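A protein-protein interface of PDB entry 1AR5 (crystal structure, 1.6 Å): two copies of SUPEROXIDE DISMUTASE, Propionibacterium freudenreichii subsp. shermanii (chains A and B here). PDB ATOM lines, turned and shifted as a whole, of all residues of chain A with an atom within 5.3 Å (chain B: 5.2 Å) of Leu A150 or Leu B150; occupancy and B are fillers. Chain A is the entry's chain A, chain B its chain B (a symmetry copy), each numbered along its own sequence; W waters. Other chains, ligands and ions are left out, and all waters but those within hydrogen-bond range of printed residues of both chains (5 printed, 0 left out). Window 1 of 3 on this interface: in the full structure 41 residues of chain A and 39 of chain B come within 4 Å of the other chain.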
ATOM      1  N   ALA A  66      -7.660  24.159 -15.064  1.00  0.00           N
ATOM      2  CA  ALA A  66      -6.868  25.023 -15.936  1.00  0.00           C
ATOM      3  C   ALA A  66      -7.222  24.869 -17.414  1.00  0.00           C
ATOM      4  O   ALA A  66      -7.402  25.861 -18.111  1.00  0.00           O
ATOM      5  CB  ALA A  66      -5.380  24.778 -15.719  1.00  0.00           C
ATOM      6  N   ALA A  70      -9.401  27.835 -19.033  1.00  0.00           N
ATOM      7  CA  ALA A  70      -8.628  28.549 -20.044  1.00  0.00           C
ATOM      8  C   ALA A  70      -9.372  28.483 -21.372  1.00  0.00           C
ATOM      9  O   ALA A  70      -9.392  29.453 -22.120  1.00  0.00           O
ATOM     10  CB  ALA A  70      -7.247  27.948 -20.185  1.00  0.00           C
ATOM     11  N   LEU A 141       1.988  36.348 -27.537  1.00  0.00           N
ATOM     12  CA  LEU A 141       2.268  35.082 -26.880  1.00  0.00           C
ATOM     13  C   LEU A 141       1.696  33.960 -27.733  1.00  0.00           C
ATOM     14  O   LEU A 141       0.747  34.163 -28.492  1.00  0.00           O
ATOM     15  CB  LEU A 141       1.634  35.033 -25.486  1.00  0.00           C
ATOM     16  CG  LEU A 141       2.180  35.968 -24.403  1.00  0.00           C
ATOM     17  CD1 LEU A 141       1.424  35.722 -23.107  1.00  0.00           C
ATOM     18  CD2 LEU A 141       3.673  35.743 -24.197  1.00  0.00           C
ATOM     19  N   PHE A 143       0.117  30.460 -27.102  1.00  0.00           N
ATOM     20  CA  PHE A 143      -0.425  29.496 -26.146  1.00  0.00           C
ATOM     21  C   PHE A 143      -0.392  28.099 -26.765  1.00  0.00           C
ATOM     22  O   PHE A 143      -0.575  27.951 -27.978  1.00  0.00           O
ATOM     23  CB  PHE A 143      -1.906  29.780 -25.815  1.00  0.00           C
ATOM     24  CG  PHE A 143      -2.178  31.104 -25.131  1.00  0.00           C
ATOM     25  CD1 PHE A 143      -1.158  32.003 -24.830  1.00  0.00           C
ATOM     26  CD2 PHE A 143      -3.487  31.452 -24.808  1.00  0.00           C
ATOM     27  CE1 PHE A 143      -1.442  33.225 -24.220  1.00  0.00           C
ATOM     28  CE2 PHE A 143      -3.781  32.669 -24.198  1.00  0.00           C
ATOM     29  CZ  PHE A 143      -2.757  33.558 -23.904  1.00  0.00           C
ATOM     30  N   HIS A 146      -4.759  25.387 -24.372  1.00  0.00           N
ATOM     31  CA  HIS A 146      -5.495  26.580 -23.939  1.00  0.00           C
ATOM     32  C   HIS A 146      -4.810  27.259 -22.766  1.00  0.00           C
ATOM     33  O   HIS A 146      -4.864  28.484 -22.622  1.00  0.00           O
ATOM     34  CB  HIS A 146      -6.900  26.224 -23.435  1.00  0.00           C
ATOM     35  CG  HIS A 146      -7.838  25.750 -24.496  1.00  0.00           C
ATOM     36  ND1 HIS A 146      -8.632  24.635 -24.337  1.00  0.00           N
ATOM     37  CD2 HIS A 146      -8.123  26.243 -25.721  1.00  0.00           C
ATOM     38  CE1 HIS A 146      -9.361  24.462 -25.421  1.00  0.00           C
ATOM     39  NE2 HIS A 146      -9.072  25.424 -26.277  1.00  0.00           N
ATOM     40  N   GLN A 147      -4.106  26.447 -21.986  1.00  0.00           N
ATOM     41  CA  GLN A 147      -3.504  26.870 -20.736  1.00  0.00           C
ATOM     42  C   GLN A 147      -1.983  26.821 -20.565  1.00  0.00           C
ATOM     43  O   GLN A 147      -1.487  26.951 -19.439  1.00  0.00           O
ATOM     44  CB  GLN A 147      -4.166  26.042 -19.624  1.00  0.00           C
ATOM     45  CG  GLN A 147      -3.656  24.580 -19.464  1.00  0.00           C
ATOM     46  CD  GLN A 147      -4.032  23.586 -20.585  1.00  0.00           C
ATOM     47  OE1 GLN A 147      -3.630  22.421 -20.534  1.00  0.00           O
ATOM     48  NE2 GLN A 147      -4.816  24.021 -21.560  1.00  0.00           N
ATOM     49  N   ASN A 148      -1.242  26.656 -21.653  1.00  0.00           N
ATOM     50  CA  ASN A 148       0.212  26.581 -21.546  1.00  0.00           C
ATOM     51  C   ASN A 148       0.962  27.668 -22.306  1.00  0.00           C
ATOM     52  O   ASN A 148       0.448  28.236 -23.268  1.00  0.00           O
ATOM     53  CB  ASN A 148       0.711  25.204 -22.007  1.00  0.00           C
ATOM     54  CG  ASN A 148       0.148  24.064 -21.180  1.00  0.00           C
ATOM     55  OD1 ASN A 148      -0.002  24.172 -19.963  1.00  0.00           O
ATOM     56  ND2 ASN A 148      -0.178  22.961 -21.842  1.00  0.00           N
ATOM     57  N   ASN A 149       2.175  27.960 -21.834  1.00  0.00           N
ATOM     58  CA  ASN A 149       3.076  28.939 -22.441  1.00  0.00           C
ATOM     59  C   ASN A 149       2.678  30.409 -22.261  1.00  0.00           C
ATOM     60  O   ASN A 149       2.734  31.196 -23.206  1.00  0.00           O
ATOM     61  CB  ASN A 149       3.275  28.603 -23.931  1.00  0.00           C
ATOM     62  CG  ASN A 149       4.655  28.983 -24.448  1.00  0.00           C
ATOM     63  OD1 ASN A 149       4.792  29.493 -25.563  1.00  0.00           O
ATOM     64  ND2 ASN A 149       5.685  28.709 -23.655  1.00  0.00           N
ATOM     65  N   LEU A 150       2.311  30.784 -21.035  1.00  0.00           N
ATOM     66  CA  LEU A 150       1.925  32.167 -20.744  1.00  0.00           C
ATOM     67  C   LEU A 150       2.183  32.537 -19.286  1.00  0.00           C
ATOM     68  O   LEU A 150       2.075  31.693 -18.394  1.00  0.00           O
ATOM     69  CB  LEU A 150       0.441  32.414 -21.064  1.00  0.00           C
ATOM     70  CG  LEU A 150      -0.618  31.776 -20.156  1.00  0.00           C
ATOM     71  CD1 LEU A 150      -1.912  32.567 -20.217  1.00  0.00           C
ATOM     72  CD2 LEU A 150      -0.850  30.335 -20.543  1.00  0.00           C
ATOM     73  N   PRO A 151       2.582  33.794 -19.035  1.00  0.00           N
ATOM     74  CA  PRO A 151       2.854  34.278 -17.679  1.00  0.00           C
ATOM     75  C   PRO A 151       1.552  34.585 -16.948  1.00  0.00           C
ATOM     76  O   PRO A 151       0.559  34.964 -17.570  1.00  0.00           O
ATOM     77  CB  PRO A 151       3.631  35.574 -17.925  1.00  0.00           C
ATOM     78  CG  PRO A 151       4.217  35.392 -19.295  1.00  0.00           C
ATOM     79  CD  PRO A 151       3.078  34.757 -20.032  1.00  0.00           C
ATOM     80  N   ALA A 152       1.554  34.413 -15.632  1.00  0.00           N
ATOM     81  CA  ALA A 152       0.375  34.714 -14.833  1.00  0.00           C
ATOM     82  C   ALA A 152       0.193  36.225 -14.897  1.00  0.00           C
ATOM     83  O   ALA A 152       1.173  36.965 -14.997  1.00  0.00           O
ATOM     84  CB  ALA A 152       0.580  34.269 -13.395  1.00  0.00           C
ATOM     85  N   SER A 154      -1.262  37.824 -17.354  1.00  0.00           N
ATOM     86  CA  SER A 154      -1.420  38.237 -18.752  1.00  0.00           C
ATOM     87  C   SER A 154      -2.886  38.537 -19.046  1.00  0.00           C
ATOM     88  O   SER A 154      -3.763  37.723 -18.751  1.00  0.00           O
ATOM     89  CB  SER A 154      -0.944  37.131 -19.696  1.00  0.00           C
ATOM     90  OG  SER A 154       0.441  36.887 -19.550  1.00  0.00           O
ATOM     91  N   ALA B  66       7.775  33.557 -22.621  1.00  0.00           N
ATOM     92  CA  ALA B  66       6.834  33.022 -21.639  1.00  0.00           C
ATOM     93  C   ALA B  66       7.521  32.402 -20.426  1.00  0.00           C
ATOM     94  O   ALA B  66       7.147  32.691 -19.293  1.00  0.00           O
ATOM     95  CB  ALA B  66       5.895  32.012 -22.293  1.00  0.00           C
ATOM     96  N   ALA B  70       7.468  34.601 -17.030  1.00  0.00           N
ATOM     97  CA  ALA B  70       6.678  33.937 -15.995  1.00  0.00           C
ATOM     98  C   ALA B  70       7.559  33.687 -14.766  1.00  0.00           C
ATOM     99  O   ALA B  70       7.089  33.776 -13.636  1.00  0.00           O
ATOM    100  CB  ALA B  70       6.096  32.627 -16.506  1.00  0.00           C
ATOM    101  N   LEU B 141      -4.393  27.042  -8.242  1.00  0.00           N
ATOM    102  CA  LEU B 141      -3.894  26.492  -9.494  1.00  0.00           C
ATOM    103  C   LEU B 141      -2.545  25.848  -9.213  1.00  0.00           C
ATOM    104  O   LEU B 141      -1.867  26.195  -8.243  1.00  0.00           O
ATOM    105  CB  LEU B 141      -3.724  27.587 -10.551  1.00  0.00           C
ATOM    106  CG  LEU B 141      -4.962  28.281 -11.133  1.00  0.00           C
ATOM    107  CD1 LEU B 141      -4.516  29.390 -12.077  1.00  0.00           C
ATOM    108  CD2 LEU B 141      -5.844  27.283 -11.869  1.00  0.00           C
ATOM    109  N   PHE B 143       0.814  25.382 -11.190  1.00  0.00           N
ATOM    110  CA  PHE B 143       1.617  25.708 -12.373  1.00  0.00           C
ATOM    111  C   PHE B 143       2.676  24.638 -12.629  1.00  0.00           C
ATOM    112  O   PHE B 143       3.197  24.040 -11.688  1.00  0.00           O
ATOM    113  CB  PHE B 143       2.385  27.032 -12.204  1.00  0.00           C
ATOM    114  CG  PHE B 143       1.523  28.256 -11.986  1.00  0.00           C
ATOM    115  CD1 PHE B 143       0.134  28.200 -12.034  1.00  0.00           C
ATOM    116  CD2 PHE B 143       2.130  29.480 -11.722  1.00  0.00           C
ATOM    117  CE1 PHE B 143      -0.634  29.347 -11.822  1.00  0.00           C
ATOM    118  CE2 PHE B 143       1.373  30.626 -11.511  1.00  0.00           C
ATOM    119  CZ  PHE B 143      -0.012  30.560 -11.561  1.00  0.00           C
ATOM    120  N   HIS B 146       7.034  27.397 -14.963  1.00  0.00           N
ATOM    121  CA  HIS B 146       6.637  28.751 -14.556  1.00  0.00           C
ATOM    122  C   HIS B 146       5.429  29.244 -15.341  1.00  0.00           C
ATOM    123  O   HIS B 146       4.607  30.004 -14.826  1.00  0.00           O
ATOM    124  CB  HIS B 146       7.748  29.768 -14.843  1.00  0.00           C
ATOM    125  CG  HIS B 146       8.970  29.594 -14.006  1.00  0.00           C
ATOM    126  ND1 HIS B 146      10.241  29.608 -14.541  1.00  0.00           N
ATOM    127  CD2 HIS B 146       9.125  29.421 -12.675  1.00  0.00           C
ATOM    128  CE1 HIS B 146      11.122  29.447 -13.573  1.00  0.00           C
ATOM    129  NE2 HIS B 146      10.471  29.332 -12.430  1.00  0.00           N
ATOM    130  N   GLN B 147       5.316  28.753 -16.573  1.00  0.00           N
ATOM    131  CA  GLN B 147       4.318  29.211 -17.523  1.00  0.00           C
ATOM    132  C   GLN B 147       3.237  28.257 -18.024  1.00  0.00           C
ATOM    133  O   GLN B 147       2.535  28.584 -18.984  1.00  0.00           O
ATOM    134  CB  GLN B 147       5.071  29.786 -18.732  1.00  0.00           C
ATOM    135  CG  GLN B 147       5.648  28.747 -19.731  1.00  0.00           C
ATOM    136  CD  GLN B 147       6.798  27.866 -19.213  1.00  0.00           C
ATOM    137  OE1 GLN B 147       7.225  26.943 -19.908  1.00  0.00           O
ATOM    138  NE2 GLN B 147       7.326  28.167 -18.033  1.00  0.00           N
ATOM    139  N   ASN B 148       3.071  27.107 -17.380  1.00  0.00           N
ATOM    140  CA  ASN B 148       2.069  26.145 -17.832  1.00  0.00           C
ATOM    141  C   ASN B 148       0.992  25.833 -16.811  1.00  0.00           C
ATOM    142  O   ASN B 148       1.186  26.019 -15.610  1.00  0.00           O
ATOM    143  CB  ASN B 148       2.739  24.831 -18.259  1.00  0.00           C
ATOM    144  CG  ASN B 148       3.747  25.019 -19.384  1.00  0.00           C
ATOM    145  OD1 ASN B 148       3.573  25.869 -20.253  1.00  0.00           O
ATOM    146  ND2 ASN B 148       4.808  24.218 -19.366  1.00  0.00           N
ATOM    147  N   ASN B 149      -0.151  25.375 -17.317  1.00  0.00           N
ATOM    148  CA  ASN B 149      -1.300  24.972 -16.508  1.00  0.00           C
ATOM    149  C   ASN B 149      -2.052  26.110 -15.815  1.00  0.00           C
ATOM    150  O   ASN B 149      -2.415  26.003 -14.640  1.00  0.00           O
ATOM    151  CB  ASN B 149      -0.875  23.901 -15.489  1.00  0.00           C
ATOM    152  CG  ASN B 149      -1.980  22.903 -15.187  1.00  0.00           C
ATOM    153  OD1 ASN B 149      -2.164  22.491 -14.043  1.00  0.00           O
ATOM    154  ND2 ASN B 149      -2.709  22.493 -16.219  1.00  0.00           N
ATOM    155  N   LEU B 150      -2.323  27.181 -16.557  1.00  0.00           N
ATOM    156  CA  LEU B 150      -3.053  28.324 -16.004  1.00  0.00           C
ATOM    157  C   LEU B 150      -3.810  29.108 -17.076  1.00  0.00           C
ATOM    158  O   LEU B 150      -3.362  29.205 -18.221  1.00  0.00           O
ATOM    159  CB  LEU B 150      -2.104  29.282 -15.270  1.00  0.00           C
ATOM    160  CG  LEU B 150      -1.144  30.134 -16.107  1.00  0.00           C
ATOM    161  CD1 LEU B 150      -0.726  31.363 -15.319  1.00  0.00           C
ATOM    162  CD2 LEU B 150       0.063  29.324 -16.525  1.00  0.00           C
ATOM    163  N   PRO B 151      -4.984  29.655 -16.718  1.00  0.00           N
ATOM    164  CA  PRO B 151      -5.797  30.440 -17.655  1.00  0.00           C
ATOM    165  C   PRO B 151      -5.286  31.878 -17.763  1.00  0.00           C
ATOM    166  O   PRO B 151      -4.815  32.457 -16.778  1.00  0.00           O
ATOM    167  CB  PRO B 151      -7.186  30.430 -17.002  1.00  0.00           C
ATOM    168  CG  PRO B 151      -7.151  29.253 -16.064  1.00  0.00           C
ATOM    169  CD  PRO B 151      -5.760  29.336 -15.511  1.00  0.00           C
ATOM    170  N   ALA B 152      -5.383  32.453 -18.956  1.00  0.00           N
ATOM    171  CA  ALA B 152      -4.963  33.833 -19.163  1.00  0.00           C
ATOM    172  C   ALA B 152      -5.857  34.725 -18.304  1.00  0.00           C
ATOM    173  O   ALA B 152      -7.040  34.430 -18.113  1.00  0.00           O
ATOM    174  CB  ALA B 152      -5.098  34.213 -20.630  1.00  0.00           C
ATOM    175  N   SER B 154      -5.400  35.265 -15.066  1.00  0.00           N
ATOM    176  CA  SER B 154      -5.286  34.860 -13.665  1.00  0.00           C
ATOM    177  C   SER B 154      -4.402  35.851 -12.909  1.00  0.00           C
ATOM    178  O   SER B 154      -3.278  36.123 -13.331  1.00  0.00           O
ATOM    179  CB  SER B 154      -4.652  33.470 -13.569  1.00  0.00           C
ATOM    180  OG  SER B 154      -5.440  32.491 -14.220  1.00  0.00           O
HETATM  181  O   HOH W   1      -1.494  22.031 -18.690  1.00  0.00           O
HETATM  182  O   HOH W   2      -5.868  30.879 -21.296  1.00  0.00           O
HETATM  183  O   HOH W   3       5.674  26.359 -22.208  1.00  0.00           O
HETATM  184  O   HOH W   4       3.421  32.651 -14.323  1.00  0.00           O
HETATM  185  O   HOH W   5      -2.466  34.536 -16.836  1.00  0.00           O
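The backbone carbonyl oxygen (O) of Gln A147 sits at hydrogen-bond distance from the backbone NH (N) of Asn B149 (3.0 Å). N of Leu B150 is in hydrogen-bond range of O of Gln A147 (3.0 Å). The backbone NH (N) of Asn B149 lies within hydrogen-bond range of the side-chain amide oxygen (OD1) of Asn A148 (2.9 Å). The backbone NH (N) of Asn A149 is in hydrogen-bond range of the backbone carbonyl oxygen (O) of Gln B147, at 2.9 Å. The side-chain amide oxygen of Asn B148 lies within hydrogen-bond range of the backbone NH of Asn A149 (3.0 Å). O of Gln B147 is in hydrogen-bond range of N of Leu A150 (3.0 Å).
Water W3 lies within hydrogen-bond range of the side-chain amide nitrogen of Asn A149 (2.8 Å), the side-chain amide oxygen of Gln B147 (2.8 Å) and the side-chain amide oxygen of Asn B148 (2.9 Å). Water W1 lies within hydrogen-bond range of ND2 of Asn B149, OE1 of Gln A147 and OD1 of Asn A148. Water W2 lies within hydrogen-bond range of N of Ala B152 (2.9 Å) and O of His A146 (2.9 Å). Water W4 bridges the backbone NH (N) of Ala A152 (2.9 Å) and the backbone carbonyl oxygen (O) of His B146 (2.9 Å). Water W5 lies within hydrogen-bond range of the backbone carbonyl oxygen (O) of Pro B151 (3.1 Å) and the backbone carbonyl oxygen (O) of Pro A151 (3.1 Å).
CB of Ala A66 touches N of Leu B150 (3.98 Å). Ala A66 touches Pro B151 (O to CG, 3.97 Å). Pro B151 touches Ala A70. Asn B148 touches Gln A147. O of Gln B147 touches C of Asn A148, 3.8 Å away. OD1 of Asn A148 touches CB of Asn B148, 3.3 Å away. CD1 of Leu A150 touches CA of Ala B152 (3.5 Å). CG of Pro A151 touches O of Ala B66, at 3.99 Å. Ala A152 touches Leu B150 (CA to CD1, 3.6 Å). Ala A152 touches Ser B154.
OG of Ser A154 is in hydrogen-bond range of O of Pro A151. The backbone carbonyl oxygen (O) of Pro B151 lies within hydrogen-bond range of the side-chain hydroxyl (OG) of Ser B154, 2.6 Å away.
Hydrophobic or aromatic side chains of chain A within 4 Å of the printed part of chain B: Ala A66, Ala A70, Leu A150, Pro A151 and Ala A152. Along chain B the printed residues that touch a printed residue of chain A span positions 66 to 154. Among the printed residues, 22 pairs touch across the chains.
Ala A66 touches Pro B151, and with the chains exchanged Pro A151 touches Ala B66. Leu A150 touches its own counterpart, Leu B150. Leu A150 touches Ala B152, and with the chains exchanged Ala A152 touches Leu B150. Ala A152 touches Ser B154, and with the chains exchanged Ser A154 touches Ala B152. Positions printed for both chains: 66, 70, 141, 143, 146, 147, 148, 149, 150, 151, 152 and 154. Of the 22 pairs that touch across the chains among the printed residues, 22 have their exchanged pair printed and touching as well.
Printed residues of chain B within 4 Å of Asn A148: Gln B147, Asn B148 and Asn B149. Of the printed residues of chain B, Leu A150 touches Ala B66 (3.99 Å), Gln B147 (3.0 Å), Leu B150 (3.6 Å) and Ala B152 (3.5 Å). Printed residues of chain B within 4 Å of Pro A151: Ala B66 and Ala B70. Of the printed residues of chain B, Ser A154 touches Ala B152 (3.7 Å). Of the printed residues of chain A, Ala B70 touches Pro A151 (3.8 Å). Leu B150 touches just these residues of chain A: Ala A66, Gln A147, Leu A150 and Ala A152. The nearest printed residue of chain B that does not touch Leu A150 is Pro B151 (4.2 Å). The nearest residue of chain A that does not touch Leu B150 is Pro A151 (4.3 Å). The nearest printed residue of chain A that does not touch Pro B151 is Leu A150 (4.2 Å).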
